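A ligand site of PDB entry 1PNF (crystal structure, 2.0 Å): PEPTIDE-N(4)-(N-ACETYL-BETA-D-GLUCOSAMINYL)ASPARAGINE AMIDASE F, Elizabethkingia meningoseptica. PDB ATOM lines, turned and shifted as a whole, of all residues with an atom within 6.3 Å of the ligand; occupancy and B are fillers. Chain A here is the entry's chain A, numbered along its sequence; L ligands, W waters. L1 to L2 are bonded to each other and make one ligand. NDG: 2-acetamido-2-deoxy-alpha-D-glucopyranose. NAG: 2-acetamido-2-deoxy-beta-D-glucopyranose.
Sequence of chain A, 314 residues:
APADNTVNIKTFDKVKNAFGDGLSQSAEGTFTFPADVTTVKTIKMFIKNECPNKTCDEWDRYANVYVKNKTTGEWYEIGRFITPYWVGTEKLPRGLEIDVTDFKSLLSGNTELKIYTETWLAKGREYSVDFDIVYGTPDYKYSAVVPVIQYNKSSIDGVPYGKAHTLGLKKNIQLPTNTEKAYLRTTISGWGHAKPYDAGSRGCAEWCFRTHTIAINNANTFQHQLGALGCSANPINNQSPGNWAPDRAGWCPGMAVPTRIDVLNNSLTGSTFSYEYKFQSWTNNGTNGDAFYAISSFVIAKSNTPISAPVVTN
Trp 59 touches the ligand.
N of Tyr 62 touches C8 of NDG L1, at 3.9 Å.
CG2 of Ile 82 touches C8 of NDG L1 (3.7 Å).
CG2 of Ile 156 touches C6 of NAG L2, 3.8 Å away.
CH2 of Trp 251 touches C8 of NDG L1, 3.7 Å away.
Hydrophobic or aromatic side chains within 4 Å of the ligand: Trp 59, Ile 82, Trp 120, Ile 156, Trp 191 and Trp 251.
Within 4 Å of the ligand: Trp 59, Asp 60, Arg 61, Tyr 62, Ile 82, Glu 118, Trp 120, Ile 156, Trp 191 and Trp 251.
O of Asp 60 sits at hydrogen-bond distance from N2 of NDG L1.
The indole nitrogen (NE1) of Trp 120 sits at hydrogen-bond distance from an oxygen (O6) of NAG L2, 2.9 Å away.
OD1 of Asp 60 lies within hydrogen-bond range of O1 of NDG L1 (2.6 Å).
The indole nitrogen of Trp 191 sits at hydrogen-bond distance from an oxygen (O3) of NDG L1 (3.0 Å).
The guanidinium group of Arg 61 sits at hydrogen-bond distance from an oxygen (O7) of NAG L2 (2.9 Å).
The side-chain carboxylate (OE2) of Glu 118 is in hydrogen-bond range of an oxygen (O6) of NAG L2.
OE1 of Glu 118 lies within hydrogen-bond range of OG of Ser 155.
N of Glu 118 lies within hydrogen-bond range of O of Tyr 62 (2.8 Å).
The backbone carbonyl oxygen (O) of Gly 190 lies within hydrogen-bond range of the indole nitrogen (NE1) of Trp 251, 3.0 Å away.
OD2 of Asp 57 lies within salt-bridge range of NE of Arg 61, 2.9 Å away.
The backbone NH (N) of Ile 156 lies close to the side-chain hydroxyl (OG) of Ser 154, at 3.3 Å.
The side-chain carboxylate (OD2) of Asp 57 lies within hydrogen-bond range of the backbone NH (N) of Trp 120 (3.3 Å).
Water W8 lies within hydrogen-bond range of O7 of NDG L1 (2.7 Å) and O of Gly 190 (3.0 Å).
Water W7 lies within hydrogen-bond range of an oxygen (O3) of NDG L1, the side-chain carboxylate (OE1) of Glu 118 and the backbone NH (N) of Tyr 62.
Water W4 lies within hydrogen-bond range of OE1 of Glu 206 (2.7 Å), O7 of NDG L1 (2.9 Å) and N of Gly 192 (3.0 Å).
Water W5 lies within hydrogen-bond range of the backbone carbonyl oxygen (O) of Glu 118 (2.7 Å), the guanidinium group (NH1) of Arg 61 (2.8 Å), an oxygen (O3) of NDG L1 (3.2 Å) and the indole nitrogen (NE1) of Trp 120 (3.2 Å).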
ATOM      1  N   ASP A  57       2.113 -23.519  20.423  1.00  0.00           N
ATOM      2  CA  ASP A  57       2.662 -23.253  19.101  1.00  0.00           C
ATOM      3  C   ASP A  57       2.580 -24.659  18.476  1.00  0.00           C
ATOM      4  O   ASP A  57       3.351 -25.562  18.836  1.00  0.00           O
ATOM      5  CB  ASP A  57       4.119 -22.776  19.242  1.00  0.00           C
ATOM      6  CG  ASP A  57       4.830 -22.582  17.922  1.00  0.00           C
ATOM      7  OD1 ASP A  57       4.233 -22.839  16.849  1.00  0.00           O
ATOM      8  OD2 ASP A  57       6.011 -22.188  17.952  1.00  0.00           O
ATOM      9  N   TRP A  59       3.333 -26.031  15.628  1.00  0.00           N
ATOM     10  CA  TRP A  59       4.349 -26.576  14.725  1.00  0.00           C
ATOM     11  C   TRP A  59       5.237 -27.605  15.420  1.00  0.00           C
ATOM     12  O   TRP A  59       5.310 -27.651  16.649  1.00  0.00           O
ATOM     13  CB  TRP A  59       5.231 -25.439  14.207  1.00  0.00           C
ATOM     14  CG  TRP A  59       4.546 -24.591  13.205  1.00  0.00           C
ATOM     15  CD1 TRP A  59       3.821 -23.446  13.431  1.00  0.00           C
ATOM     16  CD2 TRP A  59       4.491 -24.841  11.811  1.00  0.00           C
ATOM     17  NE1 TRP A  59       3.318 -22.968  12.242  1.00  0.00           N
ATOM     18  CE2 TRP A  59       3.709 -23.804  11.239  1.00  0.00           C
ATOM     19  CE3 TRP A  59       5.000 -25.836  10.994  1.00  0.00           C
ATOM     20  CZ2 TRP A  59       3.439 -23.753   9.870  1.00  0.00           C
ATOM     21  CZ3 TRP A  59       4.741 -25.777   9.629  1.00  0.00           C
ATOM     22  CH2 TRP A  59       3.962 -24.745   9.079  1.00  0.00           C
ATOM     23  N   ASP A  60       5.866 -28.457  14.626  1.00  0.00           N
ATOM     24  CA  ASP A  60       6.790 -29.434  15.168  1.00  0.00           C
ATOM     25  C   ASP A  60       8.139 -28.702  15.298  1.00  0.00           C
ATOM     26  O   ASP A  60       8.885 -28.546  14.333  1.00  0.00           O
ATOM     27  CB  ASP A  60       6.882 -30.692  14.267  1.00  0.00           C
ATOM     28  CG  ASP A  60       7.216 -30.384  12.813  1.00  0.00           C
ATOM     29  OD1 ASP A  60       6.786 -29.350  12.254  1.00  0.00           O
ATOM     30  OD2 ASP A  60       7.905 -31.223  12.205  1.00  0.00           O
ATOM     31  N   ARG A  61       8.409 -28.178  16.489  1.00  0.00           N
ATOM     32  CA  ARG A  61       9.615 -27.400  16.722  1.00  0.00           C
ATOM     33  C   ARG A  61      10.817 -28.123  17.293  1.00  0.00           C
ATOM     34  O   ARG A  61      10.706 -29.089  18.029  1.00  0.00           O
ATOM     35  CB  ARG A  61       9.314 -26.224  17.637  1.00  0.00           C
ATOM     36  CG  ARG A  61       8.195 -25.315  17.204  1.00  0.00           C
ATOM     37  CD  ARG A  61       8.537 -24.529  15.982  1.00  0.00           C
ATOM     38  NE  ARG A  61       7.530 -23.475  15.810  1.00  0.00           N
ATOM     39  CZ  ARG A  61       7.402 -22.723  14.729  1.00  0.00           C
ATOM     40  NH1 ARG A  61       8.199 -22.872  13.684  1.00  0.00           N
ATOM     41  NH2 ARG A  61       6.441 -21.800  14.701  1.00  0.00           N
ATOM     42  N   TYR A  62      11.973 -27.609  16.922  1.00  0.00           N
ATOM     43  CA  TYR A  62      13.262 -28.097  17.424  1.00  0.00           C
ATOM     44  C   TYR A  62      13.317 -27.641  18.911  1.00  0.00           C
ATOM     45  O   TYR A  62      12.948 -26.501  19.227  1.00  0.00           O
ATOM     46  CB  TYR A  62      14.380 -27.417  16.611  1.00  0.00           C
ATOM     47  CG  TYR A  62      15.798 -27.690  17.046  1.00  0.00           C
ATOM     48  CD1 TYR A  62      16.385 -26.994  18.119  1.00  0.00           C
ATOM     49  CD2 TYR A  62      16.599 -28.573  16.339  1.00  0.00           C
ATOM     50  CE1 TYR A  62      17.718 -27.175  18.458  1.00  0.00           C
ATOM     51  CE2 TYR A  62      17.950 -28.762  16.669  1.00  0.00           C
ATOM     52  CZ  TYR A  62      18.497 -28.066  17.730  1.00  0.00           C
ATOM     53  OH  TYR A  62      19.845 -28.229  18.024  1.00  0.00           O
ATOM     54  N   ILE A  82      11.817 -33.160  18.947  1.00  0.00           N
ATOM     55  CA  ILE A  82      11.029 -32.315  18.077  1.00  0.00           C
ATOM     56  C   ILE A  82       9.629 -32.340  18.687  1.00  0.00           C
ATOM     57  O   ILE A  82       9.101 -33.412  18.991  1.00  0.00           O
ATOM     58  CB  ILE A  82      10.978 -32.861  16.618  1.00  0.00           C
ATOM     59  CG1 ILE A  82      12.409 -33.120  16.101  1.00  0.00           C
ATOM     60  CG2 ILE A  82      10.309 -31.849  15.712  1.00  0.00           C
ATOM     61  CD1 ILE A  82      13.305 -31.870  16.057  1.00  0.00           C
ATOM     62  N   TYR A  85       3.168 -32.069  16.527  1.00  0.00           N
ATOM     63  CA  TYR A  85       2.294 -31.060  15.941  1.00  0.00           C
ATOM     64  C   TYR A  85       1.031 -31.005  16.791  1.00  0.00           C
ATOM     65  O   TYR A  85       0.554 -32.051  17.261  1.00  0.00           O
ATOM     66  CB  TYR A  85       1.810 -31.483  14.545  1.00  0.00           C
ATOM     67  CG  TYR A  85       2.800 -31.427  13.418  1.00  0.00           C
ATOM     68  CD1 TYR A  85       3.559 -32.560  13.067  1.00  0.00           C
ATOM     69  CD2 TYR A  85       2.889 -30.297  12.602  1.00  0.00           C
ATOM     70  CE1 TYR A  85       4.358 -32.566  11.941  1.00  0.00           C
ATOM     71  CE2 TYR A  85       3.682 -30.281  11.479  1.00  0.00           C
ATOM     72  CZ  TYR A  85       4.400 -31.427  11.142  1.00  0.00           C
ATOM     73  OH  TYR A  85       5.110 -31.443   9.964  1.00  0.00           O
ATOM     74  N   GLU A 118      12.459 -23.744  19.624  1.00  0.00           N
ATOM     75  CA  GLU A 118      12.558 -22.781  18.546  1.00  0.00           C
ATOM     76  C   GLU A 118      11.150 -22.342  18.152  1.00  0.00           C
ATOM     77  O   GLU A 118      10.752 -22.451  16.986  1.00  0.00           O
ATOM     78  CB  GLU A 118      13.294 -23.400  17.370  1.00  0.00           C
ATOM     79  CG  GLU A 118      13.799 -22.388  16.351  1.00  0.00           C
ATOM     80  CD  GLU A 118      14.666 -23.028  15.286  1.00  0.00           C
ATOM     81  OE1 GLU A 118      14.837 -24.255  15.313  1.00  0.00           O
ATOM     82  OE2 GLU A 118      15.191 -22.282  14.423  1.00  0.00           O
ATOM     83  N   TRP A 120       8.103 -19.644  17.659  1.00  0.00           N
ATOM     84  CA  TRP A 120       7.977 -18.276  17.153  1.00  0.00           C
ATOM     85  C   TRP A 120       6.591 -17.688  17.423  1.00  0.00           C
ATOM     86  O   TRP A 120       6.224 -16.655  16.861  1.00  0.00           O
ATOM     87  CB  TRP A 120       8.279 -18.247  15.656  1.00  0.00           C
ATOM     88  CG  TRP A 120       9.636 -18.717  15.337  1.00  0.00           C
ATOM     89  CD1 TRP A 120       9.982 -19.842  14.648  1.00  0.00           C
ATOM     90  CD2 TRP A 120      10.868 -18.060  15.680  1.00  0.00           C
ATOM     91  NE1 TRP A 120      11.358 -19.936  14.537  1.00  0.00           N
ATOM     92  CE2 TRP A 120      11.920 -18.846  15.167  1.00  0.00           C
ATOM     93  CE3 TRP A 120      11.174 -16.898  16.387  1.00  0.00           C
ATOM     94  CZ2 TRP A 120      13.259 -18.495  15.316  1.00  0.00           C
ATOM     95  CZ3 TRP A 120      12.496 -16.547  16.534  1.00  0.00           C
ATOM     96  CH2 TRP A 120      13.526 -17.348  16.012  1.00  0.00           C
ATOM     97  N   SER A 154      20.069 -23.789  17.594  1.00  0.00           N
ATOM     98  CA  SER A 154      18.747 -23.849  16.973  1.00  0.00           C
ATOM     99  C   SER A 154      18.907 -24.727  15.749  1.00  0.00           C
ATOM    100  O   SER A 154      20.028 -25.105  15.400  1.00  0.00           O
ATOM    101  CB  SER A 154      18.259 -22.440  16.574  1.00  0.00           C
ATOM    102  OG  SER A 154      18.781 -22.021  15.317  1.00  0.00           O
ATOM    103  N   SER A 155      17.807 -25.062  15.085  1.00  0.00           N
ATOM    104  CA  SER A 155      17.887 -25.929  13.907  1.00  0.00           C
ATOM    105  C   SER A 155      18.671 -25.260  12.792  1.00  0.00           C
ATOM    106  O   SER A 155      19.466 -25.900  12.107  1.00  0.00           O
ATOM    107  CB  SER A 155      16.495 -26.304  13.419  1.00  0.00           C
ATOM    108  OG  SER A 155      15.817 -25.145  12.986  1.00  0.00           O
ATOM    109  N   ILE A 156      18.471 -23.959  12.626  1.00  0.00           N
ATOM    110  CA  ILE A 156      19.168 -23.227  11.581  1.00  0.00           C
ATOM    111  C   ILE A 156      20.577 -22.771  12.007  1.00  0.00           C
ATOM    112  O   ILE A 156      21.286 -22.105  11.239  1.00  0.00           O
ATOM    113  CB  ILE A 156      18.275 -22.090  11.009  1.00  0.00           C
ATOM    114  CG1 ILE A 156      17.855 -21.098  12.101  1.00  0.00           C
ATOM    115  CG2 ILE A 156      17.009 -22.697  10.380  1.00  0.00           C
ATOM    116  CD1 ILE A 156      18.916 -20.073  12.497  1.00  0.00           C
ATOM    117  N   GLY A 190      18.472 -32.907  10.685  1.00  0.00           N
ATOM    118  CA  GLY A 190      18.535 -32.013   9.540  1.00  0.00           C
ATOM    119  C   GLY A 190      17.320 -31.127   9.363  1.00  0.00           C
ATOM    120  O   GLY A 190      16.172 -31.563   9.630  1.00  0.00           O
ATOM    121  N   TRP A 191      17.556 -29.910   8.885  1.00  0.00           N
ATOM    122  CA  TRP A 191      16.526 -28.902   8.648  1.00  0.00           C
ATOM    123  C   TRP A 191      16.531 -28.520   7.187  1.00  0.00           C
ATOM    124  O   TRP A 191      17.584 -28.527   6.563  1.00  0.00           O
ATOM    125  CB  TRP A 191      16.831 -27.620   9.453  1.00  0.00           C
ATOM    126  CG  TRP A 191      15.736 -26.567   9.438  1.00  0.00           C
ATOM    127  CD1 TRP A 191      14.740 -26.396  10.367  1.00  0.00           C
ATOM    128  CD2 TRP A 191      15.521 -25.539   8.436  1.00  0.00           C
ATOM    129  NE1 TRP A 191      13.928 -25.350  10.009  1.00  0.00           N
ATOM    130  CE2 TRP A 191      14.380 -24.803   8.831  1.00  0.00           C
ATOM    131  CE3 TRP A 191      16.183 -25.194   7.241  1.00  0.00           C
ATOM    132  CZ2 TRP A 191      13.878 -23.725   8.090  1.00  0.00           C
ATOM    133  CZ3 TRP A 191      15.687 -24.109   6.496  1.00  0.00           C
ATOM    134  CH2 TRP A 191      14.537 -23.392   6.920  1.00  0.00           C
ATOM    135  N   GLY A 192      15.356 -28.215   6.629  1.00  0.00           N
ATOM    136  CA  GLY A 192      15.262 -27.748   5.256  1.00  0.00           C
ATOM    137  C   GLY A 192      14.754 -28.678   4.187  1.00  0.00           C
ATOM    138  O   GLY A 192      14.700 -29.892   4.359  1.00  0.00           O
ATOM    139  N   HIS A 193      14.345 -28.097   3.064  1.00  0.00           N
ATOM    140  CA  HIS A 193      13.866 -28.870   1.932  1.00  0.00           C
ATOM    141  C   HIS A 193      14.532 -28.301   0.695  1.00  0.00           C
ATOM    142  O   HIS A 193      13.918 -28.080  -0.353  1.00  0.00           O
ATOM    143  CB  HIS A 193      12.338 -28.831   1.846  1.00  0.00           C
ATOM    144  CG  HIS A 193      11.762 -27.461   1.886  1.00  0.00           C
ATOM    145  ND1 HIS A 193      10.627 -27.155   2.609  1.00  0.00           N
ATOM    146  CD2 HIS A 193      12.151 -26.303   1.298  1.00  0.00           C
ATOM    147  CE1 HIS A 193      10.339 -25.873   2.449  1.00  0.00           C
ATOM    148  NE2 HIS A 193      11.233 -25.337   1.673  1.00  0.00           N
ATOM    149  N   GLU A 206      16.047 -32.048   5.894  1.00  0.00           N
ATOM    150  CA  GLU A 206      14.985 -32.690   6.660  1.00  0.00           C
ATOM    151  C   GLU A 206      14.512 -34.005   6.062  1.00  0.00           C
ATOM    152  O   GLU A 206      14.287 -35.000   6.774  1.00  0.00           O
ATOM    153  CB  GLU A 206      13.761 -31.766   6.800  1.00  0.00           C
ATOM    154  CG  GLU A 206      12.505 -32.529   7.247  1.00  0.00           C
ATOM    155  CD  GLU A 206      11.330 -31.658   7.641  1.00  0.00           C
ATOM    156  OE1 GLU A 206      11.319 -30.446   7.345  1.00  0.00           O
ATOM    157  OE2 GLU A 206      10.386 -32.200   8.237  1.00  0.00           O
ATOM    158  N   TRP A 251      14.738 -38.617  12.246  1.00  0.00           N
ATOM    159  CA  TRP A 251      13.930 -38.020  13.302  1.00  0.00           C
ATOM    160  C   TRP A 251      12.463 -38.058  12.964  1.00  0.00           C
ATOM    161  O   TRP A 251      12.103 -38.379  11.825  1.00  0.00           O
ATOM    162  CB  TRP A 251      14.353 -36.566  13.664  1.00  0.00           C
ATOM    163  CG  TRP A 251      14.307 -35.439  12.591  1.00  0.00           C
ATOM    164  CD1 TRP A 251      15.342 -35.026  11.799  1.00  0.00           C
ATOM    165  CD2 TRP A 251      13.205 -34.540  12.312  1.00  0.00           C
ATOM    166  NE1 TRP A 251      14.967 -33.913  11.062  1.00  0.00           N
ATOM    167  CE2 TRP A 251      13.670 -33.601  11.356  1.00  0.00           C
ATOM    168  CE3 TRP A 251      11.893 -34.435  12.780  1.00  0.00           C
ATOM    169  CZ2 TRP A 251      12.864 -32.573  10.857  1.00  0.00           C
ATOM    170  CZ3 TRP A 251      11.087 -33.407  12.281  1.00  0.00           C
ATOM    171  CH2 TRP A 251      11.580 -32.489  11.333  1.00  0.00           C
HETATM  172  C1  NDG L   1       8.990 -27.263  10.574  1.00  0.00           C
HETATM  173  C2  NDG L   1      10.426 -26.878  11.094  1.00  0.00           C
HETATM  174  C3  NDG L   1      10.363 -25.416  11.593  1.00  0.00           C
HETATM  175  C4  NDG L   1       9.769 -24.501  10.544  1.00  0.00           C
HETATM  176  C5  NDG L   1       8.431 -25.021  10.022  1.00  0.00           C
HETATM  177  C6  NDG L   1       7.784 -24.181   8.917  1.00  0.00           C
HETATM  178  C7  NDG L   1      11.829 -28.600  12.182  1.00  0.00           C
HETATM  179  C8  NDG L   1      11.989 -29.439  13.436  1.00  0.00           C
HETATM  180  O5  NDG L   1       8.592 -26.370   9.539  1.00  0.00           O
HETATM  181  O3  NDG L   1      11.673 -24.990  11.894  1.00  0.00           O
HETATM  182  O4  NDG L   1       9.528 -23.189  11.088  1.00  0.00           O
HETATM  183  O6  NDG L   1       8.562 -24.125   7.764  1.00  0.00           O
HETATM  184  O7  NDG L   1      12.636 -28.650  11.241  1.00  0.00           O
HETATM  185  N2  NDG L   1      10.801 -27.752  12.200  1.00  0.00           N
HETATM  186  O1  NDG L   1       8.013 -27.118  11.540  1.00  0.00           O
HETATM  187  C1  NAG L   2      10.268 -22.167  10.535  1.00  0.00           C
HETATM  188  C2  NAG L   2       9.532 -20.853  10.755  1.00  0.00           C
HETATM  189  C3  NAG L   2      10.416 -19.714  10.270  1.00  0.00           C
HETATM  190  C4  NAG L   2      11.786 -19.771  10.941  1.00  0.00           C
HETATM  191  C5  NAG L   2      12.422 -21.147  10.737  1.00  0.00           C
HETATM  192  C6  NAG L   2      13.689 -21.272  11.532  1.00  0.00           C
HETATM  193  C7  NAG L   2       7.098 -20.908  10.618  1.00  0.00           C
HETATM  194  C8  NAG L   2       5.880 -20.833   9.717  1.00  0.00           C
HETATM  195  N2  NAG L   2       8.277 -20.823  10.018  1.00  0.00           N
HETATM  196  O3  NAG L   2       9.794 -18.479  10.580  1.00  0.00           O
HETATM  197  O4  NAG L   2      12.632 -18.787  10.362  1.00  0.00           O
HETATM  198  O5  NAG L   2      11.533 -22.188  11.206  1.00  0.00           O
HETATM  199  O6  NAG L   2      13.438 -21.197  12.910  1.00  0.00           O
HETATM  200  O7  NAG L   2       6.975 -21.052  11.831  1.00  0.00           O
HETATM  201  O   HOH W   1       7.943 -21.152   6.151  1.00  0.00           O
HETATM  202  O   HOH W   2       8.979 -18.556   7.377  1.00  0.00           O
HETATM  203  O   HOH W   3      13.685 -16.749  11.627  1.00  0.00           O
HETATM  204  O   HOH W   4      12.852 -28.404   8.337  1.00  0.00           O
HETATM  205  O   HOH W   5      10.922 -23.140  14.381  1.00  0.00           O
HETATM  206  O   HOH W   6      12.700 -17.731   7.467  1.00  0.00           O
HETATM  207  O   HOH W   7      12.338 -25.533  14.633  1.00  0.00           O
HETATM  208  O   HOH W   8      15.034 -29.765  11.745  1.00  0.00           O
